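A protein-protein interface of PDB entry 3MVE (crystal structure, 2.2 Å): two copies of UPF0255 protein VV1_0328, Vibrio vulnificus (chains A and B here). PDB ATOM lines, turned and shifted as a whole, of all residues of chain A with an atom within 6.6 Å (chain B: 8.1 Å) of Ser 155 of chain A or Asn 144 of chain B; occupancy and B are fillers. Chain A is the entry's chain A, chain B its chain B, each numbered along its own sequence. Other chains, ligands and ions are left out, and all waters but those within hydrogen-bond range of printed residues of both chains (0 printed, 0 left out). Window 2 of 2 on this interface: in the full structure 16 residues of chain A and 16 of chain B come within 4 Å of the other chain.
The side-chain hydroxyl (OH) of Tyr 93 of chain B is in hydrogen-bond range of the side-chain amide nitrogen (NE2) of Gln 110 of chain A (2.9 Å). NE2 of Gln 110 of chain A lies within hydrogen-bond range of OE1 of Gln 148 of chain B. The side-chain amide nitrogen of Gln 148 of chain B sits at hydrogen-bond distance from the backbone carbonyl oxygen of Leu 152 of chain A (3.5 Å). The side-chain hydroxyl of Ser 155 of chain A is in hydrogen-bond range of the side-chain amide oxygen of Asn 144 of chain B, 2.9 Å away. The side-chain amide nitrogen (ND2) of Asn 144 of chain B lies within hydrogen-bond range of the side-chain carboxylate (OE1) of Glu 159 of chain A, 2.6 Å away.
O of Val 151 of chain A lies within hydrogen-bond range of OG of Ser 155 of chain A, at 3.5 Å. The side-chain carboxylate (OE1) of Glu 159 of chain A is in salt-bridge range of the side-chain amino group (NZ) of Lys 162 of chain A (3.3 Å). The side-chain carboxylate (OD1) of Asp 143 of chain B sits at hydrogen-bond distance from the backbone NH (N) of Leu 145 of chain B (3.0 Å).
Of the printed residues of chain B, Gln 110 of chain A touches Tyr 93 (2.9 Å) and Gln 148 (2.8 Å). Of the printed residues of chain B, Val 151 of chain A touches Val 151 (3.6 Å). Of the printed residues of chain B, Leu 152 of chain A touches Gln 148 (3.4 Å) and Val 151 (3.5 Å). Ser 155 of chain A touches just these residues of chain B: Asn 144 and Gln 148. Of chain B, only Gln 148 (3.96 Å) comes within 4 Å of Ala 156 of chain A. Of chain A, only Ser 155 and Glu 159 come within 4 Å of Asn 144 of chain B. The nearest residue of chain A that does not touch Asn 144 of chain B is Leu 158 of chain A (4.1 Å).
Of the 18 printed residues of chain B, 5 touch a printed residue of chain A. Printed residues of chain B that touch a printed residue of chain A: Tyr 93, Asn 144, Leu 145, Gln 148 and Val 151. Hydrophobic or aromatic side chains of chain B within 4 Å of the printed part of chain A: Tyr 93, Leu 145 and Val 151. Of the 15 printed residues of chain A, 6 touch a printed residue of chain B. Hydrophobic or aromatic side chains of chain A that line the printed part of chain B: Val 151 and Leu 152. Among the printed residues, no Asp or Glu carboxylate lies within 4 Å of a Lys or Arg side-chain nitrogen of the other chain.
Among the printed residues, pairs that only touch across the chains: Val 151 of chain A with Val 151 of chain B (3.6 Å), Leu 152 of chain A with Val 151 of chain B (3.5 Å), Ser 155 of chain A with Gln 148 of chain B (3.6 Å), Ala 156 of chain A with Gln 148 of chain B (3.96 Å) and Glu 159 of chain A with Leu 145 of chain B (3.6 Å).
Val 151 of chain B touches its own counterpart, Val 151 of chain A. 2 positions are printed for both chains. Of the 10 pairs that touch across the chains among the printed residues, 1 has its exchanged pair printed and touching as well.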
ATOM      1  N   GLN A 110      16.097   6.208   1.902  1.00  0.00           N
ATOM      2  CA  GLN A 110      14.994   5.288   2.082  1.00  0.00           C
ATOM      3  C   GLN A 110      15.430   3.876   1.705  1.00  0.00           C
ATOM      4  O   GLN A 110      15.100   2.922   2.396  1.00  0.00           O
ATOM      5  CB  GLN A 110      13.777   5.694   1.248  1.00  0.00           C
ATOM      6  CG  GLN A 110      12.553   4.825   1.571  1.00  0.00           C
ATOM      7  CD  GLN A 110      11.260   5.417   1.083  1.00  0.00           C
ATOM      8  OE1 GLN A 110      11.048   6.634   1.164  1.00  0.00           O
ATOM      9  NE2 GLN A 110      10.374   4.564   0.583  1.00  0.00           N
ATOM     10  N   SER A 129      12.846  11.345   5.113  1.00  0.00           N
ATOM     11  CA  SER A 129      11.729  12.244   5.332  1.00  0.00           C
ATOM     12  C   SER A 129      12.173  13.702   5.241  1.00  0.00           C
ATOM     13  O   SER A 129      11.551  14.507   4.542  1.00  0.00           O
ATOM     14  CB  SER A 129      11.107  11.977   6.698  1.00  0.00           C
ATOM     15  OG  SER A 129      10.002  12.826   6.911  1.00  0.00           O
ATOM     16  N   GLN A 150       5.752  16.554  -0.091  1.00  0.00           N
ATOM     17  CA  GLN A 150       5.214  16.611   1.264  1.00  0.00           C
ATOM     18  C   GLN A 150       4.600  15.251   1.617  1.00  0.00           C
ATOM     19  O   GLN A 150       4.683  14.785   2.766  1.00  0.00           O
ATOM     20  CB  GLN A 150       4.153  17.707   1.333  1.00  0.00           C
ATOM     21  CG  GLN A 150       3.964  18.354   2.674  1.00  0.00           C
ATOM     22  CD  GLN A 150       3.058  19.579   2.589  1.00  0.00           C
ATOM     23  OE1 GLN A 150       3.310  20.512   1.809  1.00  0.00           O
ATOM     24  NE2 GLN A 150       2.001  19.583   3.395  1.00  0.00           N
ATOM     25  N   VAL A 151       3.975  14.612   0.628  1.00  0.00           N
ATOM     26  CA  VAL A 151       3.392  13.296   0.854  1.00  0.00           C
ATOM     27  C   VAL A 151       4.516  12.309   1.136  1.00  0.00           C
ATOM     28  O   VAL A 151       4.399  11.455   2.013  1.00  0.00           O
ATOM     29  CB  VAL A 151       2.595  12.796  -0.377  1.00  0.00           C
ATOM     30  CG1 VAL A 151       1.976  11.435  -0.084  1.00  0.00           C
ATOM     31  CG2 VAL A 151       1.501  13.809  -0.728  1.00  0.00           C
ATOM     32  N   LEU A 152       5.608  12.422   0.388  1.00  0.00           N
ATOM     33  CA  LEU A 152       6.738  11.520   0.586  1.00  0.00           C
ATOM     34  C   LEU A 152       7.338  11.745   1.969  1.00  0.00           C
ATOM     35  O   LEU A 152       7.757  10.796   2.647  1.00  0.00           O
ATOM     36  CB  LEU A 152       7.813  11.756  -0.478  1.00  0.00           C
ATOM     37  CG  LEU A 152       7.375  11.492  -1.922  1.00  0.00           C
ATOM     38  CD1 LEU A 152       8.560  11.761  -2.834  1.00  0.00           C
ATOM     39  CD2 LEU A 152       6.881  10.058  -2.088  1.00  0.00           C
ATOM     40  N   ALA A 153       7.385  13.011   2.372  1.00  0.00           N
ATOM     41  CA  ALA A 153       7.937  13.376   3.677  1.00  0.00           C
ATOM     42  C   ALA A 153       7.105  12.744   4.781  1.00  0.00           C
ATOM     43  O   ALA A 153       7.633  12.095   5.683  1.00  0.00           O
ATOM     44  CB  ALA A 153       7.951  14.916   3.843  1.00  0.00           C
ATOM     45  N   ASN A 154       5.793  12.933   4.704  1.00  0.00           N
ATOM     46  CA  ASN A 154       4.921  12.387   5.725  1.00  0.00           C
ATOM     47  C   ASN A 154       4.922  10.866   5.789  1.00  0.00           C
ATOM     48  O   ASN A 154       4.956  10.309   6.876  1.00  0.00           O
ATOM     49  CB  ASN A 154       3.509  12.950   5.559  1.00  0.00           C
ATOM     50  CG  ASN A 154       3.418  14.411   6.005  1.00  0.00           C
ATOM     51  OD1 ASN A 154       3.979  14.783   7.037  1.00  0.00           O
ATOM     52  ND2 ASN A 154       2.700  15.234   5.244  1.00  0.00           N
ATOM     53  N   SER A 155       4.904  10.183   4.645  1.00  0.00           N
ATOM     54  CA  SER A 155       4.935   8.713   4.660  1.00  0.00           C
ATOM     55  C   SER A 155       6.245   8.172   5.236  1.00  0.00           C
ATOM     56  O   SER A 155       6.245   7.188   5.995  1.00  0.00           O
ATOM     57  CB  SER A 155       4.737   8.149   3.250  1.00  0.00           C
ATOM     58  OG  SER A 155       3.375   8.227   2.866  1.00  0.00           O
ATOM     59  N   ALA A 156       7.363   8.801   4.879  1.00  0.00           N
ATOM     60  CA  ALA A 156       8.657   8.348   5.397  1.00  0.00           C
ATOM     61  C   ALA A 156       8.742   8.590   6.904  1.00  0.00           C
ATOM     62  O   ALA A 156       9.270   7.767   7.652  1.00  0.00           O
ATOM     63  CB  ALA A 156       9.823   9.068   4.674  1.00  0.00           C
ATOM     64  N   TYR A 157       8.213   9.717   7.354  1.00  0.00           N
ATOM     65  CA  TYR A 157       8.246  10.041   8.780  1.00  0.00           C
ATOM     66  C   TYR A 157       7.502   8.964   9.570  1.00  0.00           C
ATOM     67  O   TYR A 157       7.958   8.524  10.625  1.00  0.00           O
ATOM     68  CB  TYR A 157       7.594  11.398   9.034  1.00  0.00           C
ATOM     69  CG  TYR A 157       8.058  12.077  10.310  1.00  0.00           C
ATOM     70  CD1 TYR A 157       9.295  12.724  10.367  1.00  0.00           C
ATOM     71  CD2 TYR A 157       7.245  12.103  11.446  1.00  0.00           C
ATOM     72  CE1 TYR A 157       9.717  13.398  11.534  1.00  0.00           C
ATOM     73  CE2 TYR A 157       7.652  12.768  12.615  1.00  0.00           C
ATOM     74  CZ  TYR A 157       8.884  13.419  12.648  1.00  0.00           C
ATOM     75  OH  TYR A 157       9.255  14.130  13.770  1.00  0.00           O
ATOM     76  N   LEU A 158       6.345   8.551   9.067  1.00  0.00           N
ATOM     77  CA  LEU A 158       5.578   7.506   9.746  1.00  0.00           C
ATOM     78  C   LEU A 158       6.310   6.155   9.750  1.00  0.00           C
ATOM     79  O   LEU A 158       6.235   5.413  10.727  1.00  0.00           O
ATOM     80  CB  LEU A 158       4.197   7.352   9.100  1.00  0.00           C
ATOM     81  CG  LEU A 158       3.364   8.642   9.111  1.00  0.00           C
ATOM     82  CD1 LEU A 158       1.914   8.305   8.756  1.00  0.00           C
ATOM     83  CD2 LEU A 158       3.432   9.304  10.491  1.00  0.00           C
ATOM     84  N   GLU A 159       7.014   5.830   8.666  1.00  0.00           N
ATOM     85  CA  GLU A 159       7.751   4.562   8.614  1.00  0.00           C
ATOM     86  C   GLU A 159       8.941   4.628   9.567  1.00  0.00           C
ATOM     87  O   GLU A 159       9.345   3.613  10.141  1.00  0.00           O
ATOM     88  CB  GLU A 159       8.239   4.262   7.186  1.00  0.00           C
ATOM     89  CG  GLU A 159       7.098   3.996   6.197  1.00  0.00           C
ATOM     90  CD  GLU A 159       6.198   2.856   6.666  1.00  0.00           C
ATOM     91  OE1 GLU A 159       4.971   2.908   6.429  1.00  0.00           O
ATOM     92  OE2 GLU A 159       6.721   1.899   7.267  1.00  0.00           O
ATOM     93  N   ALA A 160       9.500   5.823   9.749  1.00  0.00           N
ATOM     94  CA  ALA A 160      10.638   5.977  10.655  1.00  0.00           C
ATOM     95  C   ALA A 160      10.172   5.764  12.092  1.00  0.00           C
ATOM     96  O   ALA A 160      10.866   5.138  12.887  1.00  0.00           O
ATOM     97  CB  ALA A 160      11.262   7.367  10.508  1.00  0.00           C
ATOM     98  N   LYS A 162       7.730   3.941  13.092  1.00  0.00           N
ATOM     99  CA  LYS A 162       7.466   2.526  13.313  1.00  0.00           C
ATOM    100  C   LYS A 162       8.739   1.786  13.707  1.00  0.00           C
ATOM    101  O   LYS A 162       8.693   0.868  14.519  1.00  0.00           O
ATOM    102  CB  LYS A 162       6.865   1.887  12.061  1.00  0.00           C
ATOM    103  CG  LYS A 162       5.473   2.389  11.725  1.00  0.00           C
ATOM    104  CD  LYS A 162       4.965   1.787  10.422  1.00  0.00           C
ATOM    105  CE  LYS A 162       3.606   2.347  10.054  1.00  0.00           C
ATOM    106  NZ  LYS A 162       3.061   1.683   8.840  1.00  0.00           N
ATOM    107  N   TYR A 234      -0.245  20.287   7.323  1.00  0.00           N
ATOM    108  CA  TYR A 234      -1.515  19.673   7.708  1.00  0.00           C
ATOM    109  C   TYR A 234      -2.603  20.702   8.017  1.00  0.00           C
ATOM    110  O   TYR A 234      -3.787  20.381   7.941  1.00  0.00           O
ATOM    111  CB  TYR A 234      -1.307  18.760   8.923  1.00  0.00           C
ATOM    112  CG  TYR A 234      -0.774  17.383   8.585  1.00  0.00           C
ATOM    113  CD1 TYR A 234      -1.602  16.401   8.036  1.00  0.00           C
ATOM    114  CD2 TYR A 234       0.557  17.050   8.842  1.00  0.00           C
ATOM    115  CE1 TYR A 234      -1.108  15.116   7.755  1.00  0.00           C
ATOM    116  CE2 TYR A 234       1.054  15.779   8.571  1.00  0.00           C
ATOM    117  CZ  TYR A 234       0.225  14.820   8.032  1.00  0.00           C
ATOM    118  OH  TYR A 234       0.737  13.570   7.785  1.00  0.00           O
ATOM    119  N   LYS B  21       1.801  -2.832  10.911  1.00  0.00           N
ATOM    120  CA  LYS B  21       0.571  -2.615  10.084  1.00  0.00           C
ATOM    121  C   LYS B  21       0.843  -2.935   8.615  1.00  0.00           C
ATOM    122  O   LYS B  21       0.802  -2.052   7.752  1.00  0.00           O
ATOM    123  CB  LYS B  21       0.088  -1.178  10.229  1.00  0.00           C
ATOM    124  N   THR B  23       0.215  -4.545   4.907  1.00  0.00           N
ATOM    125  CA  THR B  23      -0.908  -4.561   3.968  1.00  0.00           C
ATOM    126  C   THR B  23      -2.054  -5.561   4.167  1.00  0.00           C
ATOM    127  O   THR B  23      -3.218  -5.159   4.266  1.00  0.00           O
ATOM    128  CB  THR B  23      -0.394  -4.725   2.515  1.00  0.00           C
ATOM    129  OG1 THR B  23       0.609  -3.731   2.250  1.00  0.00           O
ATOM    130  CG2 THR B  23      -1.526  -4.548   1.526  1.00  0.00           C
ATOM    131  N   LEU B  26      -4.347  -4.787   7.175  1.00  0.00           N
ATOM    132  CA  LEU B  26      -4.921  -3.467   7.360  1.00  0.00           C
ATOM    133  C   LEU B  26      -6.440  -3.499   7.407  1.00  0.00           C
ATOM    134  O   LEU B  26      -7.048  -2.811   8.227  1.00  0.00           O
ATOM    135  CB  LEU B  26      -4.477  -2.513   6.244  1.00  0.00           C
ATOM    136  CG  LEU B  26      -3.012  -2.070   6.216  1.00  0.00           C
ATOM    137  CD1 LEU B  26      -2.742  -1.348   4.920  1.00  0.00           C
ATOM    138  CD2 LEU B  26      -2.701  -1.174   7.417  1.00  0.00           C
ATOM    139  N   TYR B  93       9.401  -2.818   6.987  1.00  0.00           N
ATOM    140  CA  TYR B  93       9.806  -2.228   5.718  1.00  0.00           C
ATOM    141  C   TYR B  93      11.309  -2.435   5.627  1.00  0.00           C
ATOM    142  O   TYR B  93      12.092  -1.622   6.109  1.00  0.00           O
ATOM    143  CB  TYR B  93       9.495  -0.728   5.654  1.00  0.00           C
ATOM    144  CG  TYR B  93       9.865  -0.112   4.309  1.00  0.00           C
ATOM    145  CD1 TYR B  93       9.187  -0.476   3.139  1.00  0.00           C
ATOM    146  CD2 TYR B  93      10.878   0.846   4.208  1.00  0.00           C
ATOM    147  CE1 TYR B  93       9.499   0.103   1.915  1.00  0.00           C
ATOM    148  CE2 TYR B  93      11.202   1.431   2.985  1.00  0.00           C
ATOM    149  CZ  TYR B  93      10.506   1.056   1.849  1.00  0.00           C
ATOM    150  OH  TYR B  93      10.807   1.651   0.653  1.00  0.00           O
ATOM    151  N   ALA B  99       6.505  -4.082  -0.828  1.00  0.00           N
ATOM    152  CA  ALA B  99       6.672  -2.719  -1.308  1.00  0.00           C
ATOM    153  C   ALA B  99       8.154  -2.382  -1.449  1.00  0.00           C
ATOM    154  O   ALA B  99       8.556  -1.709  -2.401  1.00  0.00           O
ATOM    155  CB  ALA B  99       5.997  -1.716  -0.340  1.00  0.00           C
ATOM    156  N   GLY B 136       2.961  -0.681  -4.713  1.00  0.00           N
ATOM    157  CA  GLY B 136       1.810  -0.266  -3.914  1.00  0.00           C
ATOM    158  C   GLY B 136       0.585  -1.158  -4.029  1.00  0.00           C
ATOM    159  O   GLY B 136      -0.314  -1.121  -3.174  1.00  0.00           O
ATOM    160  N   LEU B 140      -4.342  -0.264  -1.316  1.00  0.00           N
ATOM    161  CA  LEU B 140      -5.352  -0.070  -0.278  1.00  0.00           C
ATOM    162  C   LEU B 140      -5.214   1.382   0.215  1.00  0.00           C
ATOM    163  O   LEU B 140      -4.103   1.871   0.451  1.00  0.00           O
ATOM    164  CB  LEU B 140      -5.132  -1.049   0.886  1.00  0.00           C
ATOM    165  CG  LEU B 140      -5.230  -2.547   0.546  1.00  0.00           C
ATOM    166  CD1 LEU B 140      -5.209  -3.380   1.840  1.00  0.00           C
ATOM    167  CD2 LEU B 140      -6.521  -2.824  -0.230  1.00  0.00           C
ATOM    168  N   LYS B 141      -6.345   2.065   0.349  1.00  0.00           N
ATOM    169  CA  LYS B 141      -6.363   3.458   0.788  1.00  0.00           C
ATOM    170  C   LYS B 141      -5.574   3.717   2.079  1.00  0.00           C
ATOM    171  O   LYS B 141      -4.854   4.704   2.186  1.00  0.00           O
ATOM    172  CB  LYS B 141      -7.814   3.920   0.974  1.00  0.00           C
ATOM    173  CG  LYS B 141      -8.001   5.431   1.156  1.00  0.00           C
ATOM    174  CD  LYS B 141      -7.664   6.222  -0.116  1.00  0.00           C
ATOM    175  CE  LYS B 141      -8.907   6.737  -0.864  1.00  0.00           C
ATOM    176  NZ  LYS B 141      -9.596   5.721  -1.740  1.00  0.00           N
ATOM    177  N   SER B 142      -5.697   2.819   3.047  1.00  0.00           N
ATOM    178  CA  SER B 142      -5.025   2.974   4.333  1.00  0.00           C
ATOM    179  C   SER B 142      -3.535   2.593   4.402  1.00  0.00           C
ATOM    180  O   SER B 142      -2.903   2.805   5.434  1.00  0.00           O
ATOM    181  CB  SER B 142      -5.763   2.125   5.361  1.00  0.00           C
ATOM    182  OG  SER B 142      -5.667   0.744   4.995  1.00  0.00           O
ATOM    183  N   ASP B 143      -2.998   2.012   3.324  1.00  0.00           N
ATOM    184  CA  ASP B 143      -1.614   1.536   3.267  1.00  0.00           C
ATOM    185  C   ASP B 143      -0.612   2.679   3.065  1.00  0.00           C
ATOM    186  O   ASP B 143      -0.472   3.207   1.953  1.00  0.00           O
ATOM    187  CB  ASP B 143      -1.486   0.521   2.121  1.00  0.00           C
ATOM    188  CG  ASP B 143      -0.175  -0.227   2.139  1.00  0.00           C
ATOM    189  OD1 ASP B 143       0.850   0.372   2.549  1.00  0.00           O
ATOM    190  OD2 ASP B 143      -0.170  -1.412   1.719  1.00  0.00           O
ATOM    191  N   ASN B 144       0.093   3.045   4.130  1.00  0.00           N
ATOM    192  CA  ASN B 144       1.057   4.148   4.058  1.00  0.00           C
ATOM    193  C   ASN B 144       2.111   3.946   2.966  1.00  0.00           C
ATOM    194  O   ASN B 144       2.414   4.870   2.198  1.00  0.00           O
ATOM    195  CB  ASN B 144       1.740   4.351   5.406  1.00  0.00           C
ATOM    196  CG  ASN B 144       2.754   5.478   5.373  1.00  0.00           C
ATOM    197  OD1 ASN B 144       2.415   6.619   5.061  1.00  0.00           O
ATOM    198  ND2 ASN B 144       4.010   5.162   5.678  1.00  0.00           N
ATOM    199  N   LEU B 145       2.658   2.739   2.876  1.00  0.00           N
ATOM    200  CA  LEU B 145       3.664   2.456   1.851  1.00  0.00           C
ATOM    201  C   LEU B 145       3.102   2.565   0.438  1.00  0.00           C
ATOM    202  O   LEU B 145       3.774   3.076  -0.463  1.00  0.00           O
ATOM    203  CB  LEU B 145       4.276   1.066   2.067  1.00  0.00           C
ATOM    204  CG  LEU B 145       5.118   0.961   3.346  1.00  0.00           C
ATOM    205  CD1 LEU B 145       5.501  -0.480   3.614  1.00  0.00           C
ATOM    206  CD2 LEU B 145       6.367   1.837   3.213  1.00  0.00           C
ATOM    207  N   ALA B 146       1.870   2.102   0.238  1.00  0.00           N
ATOM    208  CA  ALA B 146       1.266   2.168  -1.088  1.00  0.00           C
ATOM    209  C   ALA B 146       0.981   3.609  -1.472  1.00  0.00           C
ATOM    210  O   ALA B 146       1.112   3.988  -2.635  1.00  0.00           O
ATOM    211  CB  ALA B 146      -0.039   1.338  -1.135  1.00  0.00           C
ATOM    212  N   ILE B 147       0.582   4.412  -0.490  1.00  0.00           N
ATOM    213  CA  ILE B 147       0.296   5.817  -0.747  1.00  0.00           C
ATOM    214  C   ILE B 147       1.566   6.482  -1.244  1.00  0.00           C
ATOM    215  O   ILE B 147       1.537   7.249  -2.196  1.00  0.00           O
ATOM    216  CB  ILE B 147      -0.173   6.560   0.522  1.00  0.00           C
ATOM    217  CG1 ILE B 147      -1.493   5.967   1.024  1.00  0.00           C
ATOM    218  CG2 ILE B 147      -0.341   8.059   0.219  1.00  0.00           C
ATOM    219  CD1 ILE B 147      -2.629   6.114   0.055  1.00  0.00           C
ATOM    220  N   GLN B 148       2.681   6.181  -0.596  1.00  0.00           N
ATOM    221  CA  GLN B 148       3.945   6.779  -0.988  1.00  0.00           C
ATOM    222  C   GLN B 148       4.396   6.252  -2.353  1.00  0.00           C
ATOM    223  O   GLN B 148       4.913   7.002  -3.183  1.00  0.00           O
ATOM    224  CB  GLN B 148       5.042   6.495   0.052  1.00  0.00           C
ATOM    225  CG  GLN B 148       6.291   7.347  -0.182  1.00  0.00           C
ATOM    226  CD  GLN B 148       7.512   6.807   0.513  1.00  0.00           C
ATOM    227  OE1 GLN B 148       7.789   5.611   0.438  1.00  0.00           O
ATOM    228  NE2 GLN B 148       8.270   7.690   1.186  1.00  0.00           N
ATOM    229  N   ALA B 149       4.196   4.958  -2.577  1.00  0.00           N
ATOM    230  CA  ALA B 149       4.593   4.355  -3.840  1.00  0.00           C
ATOM    231  C   ALA B 149       3.804   4.957  -4.993  1.00  0.00           C
ATOM    232  O   ALA B 149       4.310   5.070  -6.107  1.00  0.00           O
ATOM    233  CB  ALA B 149       4.394   2.842  -3.793  1.00  0.00           C
ATOM    234  N   GLN B 150       2.563   5.348  -4.731  1.00  0.00           N
ATOM    235  CA  GLN B 150       1.738   5.941  -5.781  1.00  0.00           C
ATOM    236  C   GLN B 150       2.373   7.266  -6.197  1.00  0.00           C
ATOM    237  O   GLN B 150       2.382   7.625  -7.376  1.00  0.00           O
ATOM    238  CB  GLN B 150       0.299   6.155  -5.279  1.00  0.00           C
ATOM    239  CG  GLN B 150      -0.673   6.617  -6.357  1.00  0.00           C
ATOM    240  CD  GLN B 150      -2.136   6.502  -5.927  1.00  0.00           C
ATOM    241  OE1 GLN B 150      -2.549   5.513  -5.308  1.00  0.00           O
ATOM    242  NE2 GLN B 150      -2.925   7.503  -6.275  1.00  0.00           N
ATOM    243  N   VAL B 151       2.904   8.004  -5.230  1.00  0.00           N
ATOM    244  CA  VAL B 151       3.569   9.263  -5.559  1.00  0.00           C
ATOM    245  C   VAL B 151       4.785   8.960  -6.452  1.00  0.00           C
ATOM    246  O   VAL B 151       4.995   9.582  -7.495  1.00  0.00           O
ATOM    247  CB  VAL B 151       4.069   9.984  -4.292  1.00  0.00           C
ATOM    248  CG1 VAL B 151       4.880  11.213  -4.691  1.00  0.00           C
ATOM    249  CG2 VAL B 151       2.884  10.352  -3.397  1.00  0.00           C
